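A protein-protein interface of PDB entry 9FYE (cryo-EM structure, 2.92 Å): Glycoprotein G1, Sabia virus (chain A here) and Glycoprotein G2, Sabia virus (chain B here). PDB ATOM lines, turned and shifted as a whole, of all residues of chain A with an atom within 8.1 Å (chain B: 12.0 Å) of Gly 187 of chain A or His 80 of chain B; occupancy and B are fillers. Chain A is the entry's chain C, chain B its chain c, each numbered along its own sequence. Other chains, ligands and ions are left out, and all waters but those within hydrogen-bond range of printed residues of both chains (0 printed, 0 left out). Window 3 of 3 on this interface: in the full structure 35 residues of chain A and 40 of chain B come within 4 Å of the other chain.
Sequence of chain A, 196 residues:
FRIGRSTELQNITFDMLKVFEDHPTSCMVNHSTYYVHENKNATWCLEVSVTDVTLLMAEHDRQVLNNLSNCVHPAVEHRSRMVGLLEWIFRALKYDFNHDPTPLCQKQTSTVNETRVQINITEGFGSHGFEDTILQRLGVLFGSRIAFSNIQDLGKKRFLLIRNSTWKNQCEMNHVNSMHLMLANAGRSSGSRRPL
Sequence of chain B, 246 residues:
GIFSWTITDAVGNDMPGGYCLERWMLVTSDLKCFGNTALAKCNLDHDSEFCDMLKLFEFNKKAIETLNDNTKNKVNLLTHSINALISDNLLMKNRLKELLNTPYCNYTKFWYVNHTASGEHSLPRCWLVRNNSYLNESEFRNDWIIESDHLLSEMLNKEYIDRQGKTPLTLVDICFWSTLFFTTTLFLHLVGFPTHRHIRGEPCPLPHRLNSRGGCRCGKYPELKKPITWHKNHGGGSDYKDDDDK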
ATOM      1  N   HIS A  23      19.864  17.471 -15.235  1.00  0.00           N
ATOM      2  CA  HIS A  23      20.749  17.031 -14.174  1.00  0.00           C
ATOM      3  C   HIS A  23      21.630  18.179 -13.705  1.00  0.00           C
ATOM      4  O   HIS A  23      21.919  19.096 -14.479  1.00  0.00           O
ATOM      5  CB  HIS A  23      21.624  15.869 -14.651  1.00  0.00           C
ATOM      6  CG  HIS A  23      20.850  14.646 -15.028  1.00  0.00           C
ATOM      7  ND1 HIS A  23      20.612  14.293 -16.339  1.00  0.00           N
ATOM      8  CD2 HIS A  23      20.265  13.691 -14.269  1.00  0.00           C
ATOM      9  CE1 HIS A  23      19.908  13.176 -16.369  1.00  0.00           C
ATOM     10  NE2 HIS A  23      19.686  12.790 -15.127  1.00  0.00           N
ATOM     11  N   TRP A  88      24.723  18.021  -2.508  1.00  0.00           N
ATOM     12  CA  TRP A  88      25.512  17.730  -3.704  1.00  0.00           C
ATOM     13  C   TRP A  88      26.810  18.525  -3.734  1.00  0.00           C
ATOM     14  O   TRP A  88      27.875  17.971  -4.028  1.00  0.00           O
ATOM     15  CB  TRP A  88      24.669  18.011  -4.952  1.00  0.00           C
ATOM     16  CG  TRP A  88      23.779  16.880  -5.375  1.00  0.00           C
ATOM     17  CD1 TRP A  88      22.611  16.491  -4.800  1.00  0.00           C
ATOM     18  CD2 TRP A  88      23.899  16.116  -6.583  1.00  0.00           C
ATOM     19  NE1 TRP A  88      22.055  15.454  -5.506  1.00  0.00           N
ATOM     20  CE2 TRP A  88      22.820  15.217  -6.617  1.00  0.00           C
ATOM     21  CE3 TRP A  88      24.833  16.084  -7.621  1.00  0.00           C
ATOM     22  CZ2 TRP A  88      22.652  14.293  -7.643  1.00  0.00           C
ATOM     23  CZ3 TRP A  88      24.668  15.164  -8.635  1.00  0.00           C
ATOM     24  CH2 TRP A  88      23.586  14.282  -8.640  1.00  0.00           C
ATOM     25  N   ARG A  91      29.146  17.244  -0.741  1.00  0.00           N
ATOM     26  CA  ARG A  91      29.693  15.930  -1.056  1.00  0.00           C
ATOM     27  C   ARG A  91      30.692  16.014  -2.200  1.00  0.00           C
ATOM     28  O   ARG A  91      31.680  15.272  -2.226  1.00  0.00           O
ATOM     29  CB  ARG A  91      28.557  14.974  -1.401  1.00  0.00           C
ATOM     30  CG  ARG A  91      28.951  13.518  -1.527  1.00  0.00           C
ATOM     31  CD  ARG A  91      27.716  12.638  -1.655  1.00  0.00           C
ATOM     32  NE  ARG A  91      26.704  12.954  -0.655  1.00  0.00           N
ATOM     33  CZ  ARG A  91      25.502  13.443  -0.931  1.00  0.00           C
ATOM     34  NH1 ARG A  91      25.122  13.684  -2.174  1.00  0.00           N
ATOM     35  NH2 ARG A  91      24.658  13.691   0.066  1.00  0.00           N
ATOM     36  N   MET A 182      28.209  14.968 -10.977  1.00  0.00           N
ATOM     37  CA  MET A 182      27.511  13.687 -10.899  1.00  0.00           C
ATOM     38  C   MET A 182      28.404  12.593 -10.336  1.00  0.00           C
ATOM     39  O   MET A 182      27.947  11.766  -9.543  1.00  0.00           O
ATOM     40  CB  MET A 182      27.023  13.249 -12.272  1.00  0.00           C
ATOM     41  CG  MET A 182      25.949  14.076 -12.891  1.00  0.00           C
ATOM     42  SD  MET A 182      25.617  13.331 -14.484  1.00  0.00           S
ATOM     43  CE  MET A 182      24.628  14.601 -15.215  1.00  0.00           C
ATOM     44  N   LEU A 183      29.667  12.544 -10.758  1.00  0.00           N
ATOM     45  CA  LEU A 183      30.554  11.499 -10.266  1.00  0.00           C
ATOM     46  C   LEU A 183      30.759  11.624  -8.767  1.00  0.00           C
ATOM     47  O   LEU A 183      30.836  10.614  -8.058  1.00  0.00           O
ATOM     48  CB  LEU A 183      31.890  11.536 -11.001  1.00  0.00           C
ATOM     49  CG  LEU A 183      31.897  10.761 -12.316  1.00  0.00           C
ATOM     50  CD1 LEU A 183      33.238  10.888 -12.998  1.00  0.00           C
ATOM     51  CD2 LEU A 183      31.552   9.305 -12.080  1.00  0.00           C
ATOM     52  N   ALA A 184      30.862  12.854  -8.264  1.00  0.00           N
ATOM     53  CA  ALA A 184      30.998  13.031  -6.823  1.00  0.00           C
ATOM     54  C   ALA A 184      29.768  12.519  -6.078  1.00  0.00           C
ATOM     55  O   ALA A 184      29.892  11.874  -5.030  1.00  0.00           O
ATOM     56  CB  ALA A 184      31.252  14.498  -6.504  1.00  0.00           C
ATOM     57  N   ASN A 185      28.575  12.799  -6.596  1.00  0.00           N
ATOM     58  CA  ASN A 185      27.308  12.344  -6.021  1.00  0.00           C
ATOM     59  C   ASN A 185      26.741  11.219  -6.884  1.00  0.00           C
ATOM     60  O   ASN A 185      25.990  11.465  -7.829  1.00  0.00           O
ATOM     61  CB  ASN A 185      26.336  13.504  -5.932  1.00  0.00           C
ATOM     62  CG  ASN A 185      26.925  14.696  -5.226  1.00  0.00           C
ATOM     63  OD1 ASN A 185      27.013  14.715  -4.007  1.00  0.00           O
ATOM     64  ND2 ASN A 185      27.375  15.679  -5.990  1.00  0.00           N
ATOM     65  N   ALA A 186      27.052   9.980  -6.521  1.00  0.00           N
ATOM     66  CA  ALA A 186      26.730   8.820  -7.342  1.00  0.00           C
ATOM     67  C   ALA A 186      25.688   7.957  -6.644  1.00  0.00           C
ATOM     68  O   ALA A 186      25.843   7.617  -5.466  1.00  0.00           O
ATOM     69  CB  ALA A 186      27.985   7.999  -7.639  1.00  0.00           C
ATOM     70  N   GLY A 187      24.636   7.606  -7.373  1.00  0.00           N
ATOM     71  CA  GLY A 187      23.540   6.836  -6.810  1.00  0.00           C
ATOM     72  C   GLY A 187      22.696   7.604  -5.819  1.00  0.00           C
ATOM     73  O   GLY A 187      22.254   7.035  -4.814  1.00  0.00           O
ATOM     74  N   ARG A 188      22.463   8.890  -6.075  1.00  0.00           N
ATOM     75  CA  ARG A 188      21.789   9.761  -5.127  1.00  0.00           C
ATOM     76  C   ARG A 188      20.793  10.650  -5.852  1.00  0.00           C
ATOM     77  O   ARG A 188      20.888  10.875  -7.060  1.00  0.00           O
ATOM     78  CB  ARG A 188      22.789  10.622  -4.356  1.00  0.00           C
ATOM     79  CG  ARG A 188      23.531   9.867  -3.285  1.00  0.00           C
ATOM     80  CD  ARG A 188      24.812  10.568  -2.940  1.00  0.00           C
ATOM     81  NE  ARG A 188      25.452   9.976  -1.775  1.00  0.00           N
ATOM     82  CZ  ARG A 188      26.427   9.083  -1.835  1.00  0.00           C
ATOM     83  NH1 ARG A 188      26.911   8.665  -2.993  1.00  0.00           N
ATOM     84  NH2 ARG A 188      26.940   8.608  -0.707  1.00  0.00           N
ATOM     85  N   SER A 189      19.829  11.155  -5.088  1.00  0.00           N
ATOM     86  CA  SER A 189      18.820  12.073  -5.590  1.00  0.00           C
ATOM     87  C   SER A 189      18.739  13.268  -4.652  1.00  0.00           C
ATOM     88  O   SER A 189      19.148  13.197  -3.491  1.00  0.00           O
ATOM     89  CB  SER A 189      17.449  11.398  -5.714  1.00  0.00           C
ATOM     90  OG  SER A 189      17.515  10.263  -6.561  1.00  0.00           O
ATOM     91  N   LYS B  55      28.409   5.876 -24.810  1.00  0.00           N
ATOM     92  CA  LYS B  55      27.699   5.157 -23.756  1.00  0.00           C
ATOM     93  C   LYS B  55      26.642   6.039 -23.107  1.00  0.00           C
ATOM     94  O   LYS B  55      25.538   5.578 -22.799  1.00  0.00           O
ATOM     95  CB  LYS B  55      28.685   4.638 -22.712  1.00  0.00           C
ATOM     96  CG  LYS B  55      29.382   3.354 -23.112  1.00  0.00           C
ATOM     97  CD  LYS B  55      29.991   2.656 -21.910  1.00  0.00           C
ATOM     98  CE  LYS B  55      31.308   3.280 -21.494  1.00  0.00           C
ATOM     99  NZ  LYS B  55      32.392   2.942 -22.454  1.00  0.00           N
ATOM    100  N   LEU B  56      26.965   7.315 -22.897  1.00  0.00           N
ATOM    101  CA  LEU B  56      25.976   8.259 -22.384  1.00  0.00           C
ATOM    102  C   LEU B  56      24.805   8.415 -23.345  1.00  0.00           C
ATOM    103  O   LEU B  56      23.645   8.458 -22.921  1.00  0.00           O
ATOM    104  CB  LEU B  56      26.632   9.611 -22.121  1.00  0.00           C
ATOM    105  CG  LEU B  56      27.092   9.854 -20.689  1.00  0.00           C
ATOM    106  CD1 LEU B  56      28.147   8.857 -20.314  1.00  0.00           C
ATOM    107  CD2 LEU B  56      27.641  11.254 -20.568  1.00  0.00           C
ATOM    108  N   PHE B  59      22.662   5.259 -23.132  1.00  0.00           N
ATOM    109  CA  PHE B  59      21.883   5.276 -21.901  1.00  0.00           C
ATOM    110  C   PHE B  59      20.716   6.247 -22.005  1.00  0.00           C
ATOM    111  O   PHE B  59      19.603   5.937 -21.569  1.00  0.00           O
ATOM    112  CB  PHE B  59      22.786   5.631 -20.720  1.00  0.00           C
ATOM    113  CG  PHE B  59      22.050   5.826 -19.428  1.00  0.00           C
ATOM    114  CD1 PHE B  59      21.530   7.062 -19.083  1.00  0.00           C
ATOM    115  CD2 PHE B  59      21.873   4.766 -18.559  1.00  0.00           C
ATOM    116  CE1 PHE B  59      20.851   7.234 -17.899  1.00  0.00           C
ATOM    117  CE2 PHE B  59      21.197   4.936 -17.374  1.00  0.00           C
ATOM    118  CZ  PHE B  59      20.686   6.171 -17.045  1.00  0.00           C
ATOM    119  N   ASN B  60      20.951   7.430 -22.574  1.00  0.00           N
ATOM    120  CA  ASN B  60      19.876   8.404 -22.721  1.00  0.00           C
ATOM    121  C   ASN B  60      18.788   7.881 -23.649  1.00  0.00           C
ATOM    122  O   ASN B  60      17.595   8.069 -23.389  1.00  0.00           O
ATOM    123  CB  ASN B  60      20.437   9.727 -23.239  1.00  0.00           C
ATOM    124  CG  ASN B  60      19.430  10.854 -23.172  1.00  0.00           C
ATOM    125  OD1 ASN B  60      19.038  11.411 -24.195  1.00  0.00           O
ATOM    126  ND2 ASN B  60      19.013  11.203 -21.962  1.00  0.00           N
ATOM    127  N   LYS B  62      17.999   4.676 -24.241  1.00  0.00           N
ATOM    128  CA  LYS B  62      17.251   3.633 -23.543  1.00  0.00           C
ATOM    129  C   LYS B  62      16.346   4.227 -22.467  1.00  0.00           C
ATOM    130  O   LYS B  62      15.229   3.741 -22.251  1.00  0.00           O
ATOM    131  CB  LYS B  62      18.209   2.589 -22.962  1.00  0.00           C
ATOM    132  CG  LYS B  62      18.601   2.779 -21.507  1.00  0.00           C
ATOM    133  CD  LYS B  62      19.291   1.537 -20.966  1.00  0.00           C
ATOM    134  CE  LYS B  62      19.878   1.791 -19.591  1.00  0.00           C
ATOM    135  NZ  LYS B  62      18.851   2.288 -18.636  1.00  0.00           N
ATOM    136  N   ALA B  63      16.810   5.273 -21.775  1.00  0.00           N
ATOM    137  CA  ALA B  63      15.979   5.924 -20.767  1.00  0.00           C
ATOM    138  C   ALA B  63      14.758   6.578 -21.399  1.00  0.00           C
ATOM    139  O   ALA B  63      13.657   6.532 -20.835  1.00  0.00           O
ATOM    140  CB  ALA B  63      16.800   6.954 -19.992  1.00  0.00           C
ATOM    141  N   LEU B  77      17.997   8.162 -13.197  1.00  0.00           N
ATOM    142  CA  LEU B  77      18.676   6.892 -13.425  1.00  0.00           C
ATOM    143  C   LEU B  77      20.129   7.110 -13.839  1.00  0.00           C
ATOM    144  O   LEU B  77      20.956   6.209 -13.715  1.00  0.00           O
ATOM    145  CB  LEU B  77      17.938   6.080 -14.492  1.00  0.00           C
ATOM    146  CG  LEU B  77      18.314   4.604 -14.636  1.00  0.00           C
ATOM    147  CD1 LEU B  77      18.034   3.841 -13.348  1.00  0.00           C
ATOM    148  CD2 LEU B  77      17.578   3.974 -15.809  1.00  0.00           C
ATOM    149  N   LEU B  78      20.436   8.314 -14.331  1.00  0.00           N
ATOM    150  CA  LEU B  78      21.801   8.619 -14.748  1.00  0.00           C
ATOM    151  C   LEU B  78      22.760   8.628 -13.567  1.00  0.00           C
ATOM    152  O   LEU B  78      23.937   8.286 -13.722  1.00  0.00           O
ATOM    153  CB  LEU B  78      21.845   9.961 -15.478  1.00  0.00           C
ATOM    154  CG  LEU B  78      23.183  10.367 -16.102  1.00  0.00           C
ATOM    155  CD1 LEU B  78      23.710   9.281 -17.025  1.00  0.00           C
ATOM    156  CD2 LEU B  78      23.051  11.680 -16.851  1.00  0.00           C
ATOM    157  N   THR B  79      22.279   9.026 -12.390  1.00  0.00           N
ATOM    158  CA  THR B  79      23.135   9.064 -11.209  1.00  0.00           C
ATOM    159  C   THR B  79      23.625   7.670 -10.834  1.00  0.00           C
ATOM    160  O   THR B  79      24.784   7.497 -10.443  1.00  0.00           O
ATOM    161  CB  THR B  79      22.382   9.705 -10.045  1.00  0.00           C
ATOM    162  OG1 THR B  79      21.641  10.834 -10.521  1.00  0.00           O
ATOM    163  CG2 THR B  79      23.357  10.176  -8.993  1.00  0.00           C
ATOM    164  N   HIS B  80      22.753   6.664 -10.939  1.00  0.00           N
ATOM    165  CA  HIS B  80      23.144   5.308 -10.570  1.00  0.00           C
ATOM    166  C   HIS B  80      24.092   4.685 -11.588  1.00  0.00           C
ATOM    167  O   HIS B  80      24.876   3.797 -11.237  1.00  0.00           O
ATOM    168  CB  HIS B  80      21.904   4.430 -10.407  1.00  0.00           C
ATOM    169  CG  HIS B  80      20.960   4.904  -9.348  1.00  0.00           C
ATOM    170  ND1 HIS B  80      20.970   4.403  -8.065  1.00  0.00           N
ATOM    171  CD2 HIS B  80      19.980   5.837  -9.379  1.00  0.00           C
ATOM    172  CE1 HIS B  80      20.037   5.005  -7.351  1.00  0.00           C
ATOM    173  NE2 HIS B  80      19.421   5.881  -8.125  1.00  0.00           N
ATOM    174  N   SER B  81      24.043   5.131 -12.841  1.00  0.00           N
ATOM    175  CA  SER B  81      24.834   4.536 -13.908  1.00  0.00           C
ATOM    176  C   SER B  81      26.054   5.362 -14.288  1.00  0.00           C
ATOM    177  O   SER B  81      26.830   4.927 -15.145  1.00  0.00           O
ATOM    178  CB  SER B  81      23.962   4.323 -15.148  1.00  0.00           C
ATOM    179  OG  SER B  81      22.718   3.743 -14.805  1.00  0.00           O
ATOM    180  N   ILE B  82      26.245   6.531 -13.673  1.00  0.00           N
ATOM    181  CA  ILE B  82      27.298   7.449 -14.106  1.00  0.00           C
ATOM    182  C   ILE B  82      28.677   6.811 -13.956  1.00  0.00           C
ATOM    183  O   ILE B  82      29.566   7.030 -14.784  1.00  0.00           O
ATOM    184  CB  ILE B  82      27.185   8.788 -13.346  1.00  0.00           C
ATOM    185  CG1 ILE B  82      28.053   9.863 -14.005  1.00  0.00           C
ATOM    186  CG2 ILE B  82      27.520   8.628 -11.868  1.00  0.00           C
ATOM    187  CD1 ILE B  82      27.522  10.354 -15.330  1.00  0.00           C
ATOM    188  N   ASN B  83      28.879   6.018 -12.899  1.00  0.00           N
ATOM    189  CA  ASN B  83      30.178   5.386 -12.686  1.00  0.00           C
ATOM    190  C   ASN B  83      30.512   4.404 -13.803  1.00  0.00           C
ATOM    191  O   ASN B  83      31.654   4.354 -14.274  1.00  0.00           O
ATOM    192  CB  ASN B  83      30.202   4.675 -11.337  1.00  0.00           C
ATOM    193  CG  ASN B  83      30.225   5.635 -10.173  1.00  0.00           C
ATOM    194  OD1 ASN B  83      30.970   6.616 -10.174  1.00  0.00           O
ATOM    195  ND2 ASN B  83      29.410   5.358  -9.163  1.00  0.00           N
ATOM    196  N   ALA B  84      29.534   3.604 -14.226  1.00  0.00           N
ATOM    197  CA  ALA B  84      29.771   2.659 -15.312  1.00  0.00           C
ATOM    198  C   ALA B  84      29.928   3.370 -16.649  1.00  0.00           C
ATOM    199  O   ALA B  84      30.777   2.992 -17.463  1.00  0.00           O
ATOM    200  CB  ALA B  84      28.638   1.637 -15.373  1.00  0.00           C
ATOM    201  N   LEU B  85      29.103   4.386 -16.906  1.00  0.00           N
ATOM    202  CA  LEU B  85      29.119   5.043 -18.210  1.00  0.00           C
ATOM    203  C   LEU B  85      30.385   5.870 -18.421  1.00  0.00           C
ATOM    204  O   LEU B  85      30.905   5.935 -19.540  1.00  0.00           O
ATOM    205  CB  LEU B  85      27.873   5.910 -18.369  1.00  0.00           C
ATOM    206  CG  LEU B  85      26.529   5.193 -18.250  1.00  0.00           C
ATOM    207  CD1 LEU B  85      25.398   6.197 -18.242  1.00  0.00           C
ATOM    208  CD2 LEU B  85      26.355   4.200 -19.377  1.00  0.00           C
ATOM    209  N   ILE B  86      30.893   6.508 -17.370  1.00  0.00           N
ATOM    210  CA  ILE B  86      31.997   7.459 -17.474  1.00  0.00           C
ATOM    211  C   ILE B  86      33.217   6.911 -16.751  1.00  0.00           C
ATOM    212  O   ILE B  86      33.106   6.352 -15.655  1.00  0.00           O
ATOM    213  CB  ILE B  86      31.600   8.836 -16.904  1.00  0.00           C
ATOM    214  CG1 ILE B  86      30.579   9.513 -17.812  1.00  0.00           C
ATOM    215  CG2 ILE B  86      32.810   9.736 -16.722  1.00  0.00           C
ATOM    216  CD1 ILE B  86      31.199  10.118 -19.041  1.00  0.00           C
ATOM    217  N   SER B  87      34.386   7.082 -17.366  1.00  0.00           N
ATOM    218  CA  SER B  87      35.657   6.748 -16.733  1.00  0.00           C
ATOM    219  C   SER B  87      36.074   7.921 -15.854  1.00  0.00           C
ATOM    220  O   SER B  87      36.375   9.005 -16.358  1.00  0.00           O
ATOM    221  CB  SER B  87      36.714   6.446 -17.788  1.00  0.00           C
ATOM    222  OG  SER B  87      37.859   5.848 -17.210  1.00  0.00           O
ATOM    223  N   ASP B  88      36.080   7.706 -14.538  1.00  0.00           N
ATOM    224  CA  ASP B  88      36.406   8.782 -13.607  1.00  0.00           C
ATOM    225  C   ASP B  88      37.878   9.161 -13.703  1.00  0.00           C
ATOM    226  O   ASP B  88      38.226  10.346 -13.645  1.00  0.00           O
ATOM    227  CB  ASP B  88      36.039   8.354 -12.184  1.00  0.00           C
ATOM    228  CG  ASP B  88      36.051   9.508 -11.190  1.00  0.00           C
ATOM    229  OD1 ASP B  88      36.650  10.564 -11.471  1.00  0.00           O
ATOM    230  OD2 ASP B  88      35.447   9.352 -10.108  1.00  0.00           O
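O of Thr 79 of chain B sits at hydrogen-bond distance from N of Gly 187 of chain A (3.1 Å).
The backbone carbonyl oxygen of Trp 88 of chain A lies close to the side-chain amide nitrogen of Asn 185 of chain A, 3.1 Å away. The guanidinium group of Arg 91 of chain A lies within hydrogen-bond range of the side-chain amide oxygen of Asn 185 of chain A (2.8 Å). NH1 of Arg 188 of chain A lies within hydrogen-bond range of O of Ala 186 of chain A, at 2.9 Å.
His 23 of chain A touches Leu 78 of chain B. Leu 78 of chain B touches Met 182 of chain A (CD2 to CE, 3.7 Å). Met 182 of chain A touches Ile 82 of chain B. Leu 183 of chain A touches Asn 83 of chain B (CD2 to OD1, 3.3 Å). Leu 183 of chain A touches Ile 86 of chain B. Leu 183 of chain A touches Asp 88 of chain B (CD1 to CG, 3.6 Å). Asn 185 of chain A touches Thr 79 of chain B (O to CG2, 3.2 Å). Thr 79 of chain B touches Ala 186 of chain A (O to CA, 3.9 Å). Asn 83 of chain B touches Ala 186 of chain A. Gly 187 of chain A touches His 80 of chain B (CA to ND1, 3.8 Å).
Printed residues of chain B within 4 Å of His 23 of chain A: Leu 78 (3.5 Å). Of the printed residues of chain B, Leu 183 of chain A touches Asn 83, Ile 86 and Asp 88. Printed residues of chain B within 4 Å of Ala 186 of chain A: Thr 79 and Asn 83. Of chain B, only Thr 79 and His 80 come within 4 Å of Gly 187 of chain A. Arg 188 of chain A touches just one residue of chain B: Thr 79 (3.2 Å). No residue of chain B comes within 4 Å of Ser 189 of chain A. Of the printed residues of chain A, Leu 78 of chain B touches His 23 (3.5 Å) and Met 182 (3.7 Å). His 80 of chain B touches one residue of chain A. Printed residues of chain A within 4 Å of Asn 83 of chain B: Leu 183 and Ala 186. Leu 85 of chain B touches none of the printed residues of chain A. Ser 87 of chain B touches none of the printed residues of chain A. Printed residues of chain A within 4 Å of Asp 88 of chain B: Leu 183 (3.6 Å). The nearest residue of chain B that does not touch Gly 187 of chain A is Ile 82 of chain B (5.4 Å). The nearest printed residue of chain A that does not touch Ile 82 of chain B is Leu 183 of chain A (4.03 Å).
Hydrophobic or aromatic side chains of chain B that line the printed part of chain A: Leu 78, His 80, Ile 82 and Ile 86. Of the 11 printed residues of chain A, 7 touch a printed residue of chain B. Among the printed residues, 12 pairs touch across the chains. Among the printed residues, no Asp or Glu carboxylate lies within 4 Å of a Lys or Arg side-chain nitrogen of the other chain.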
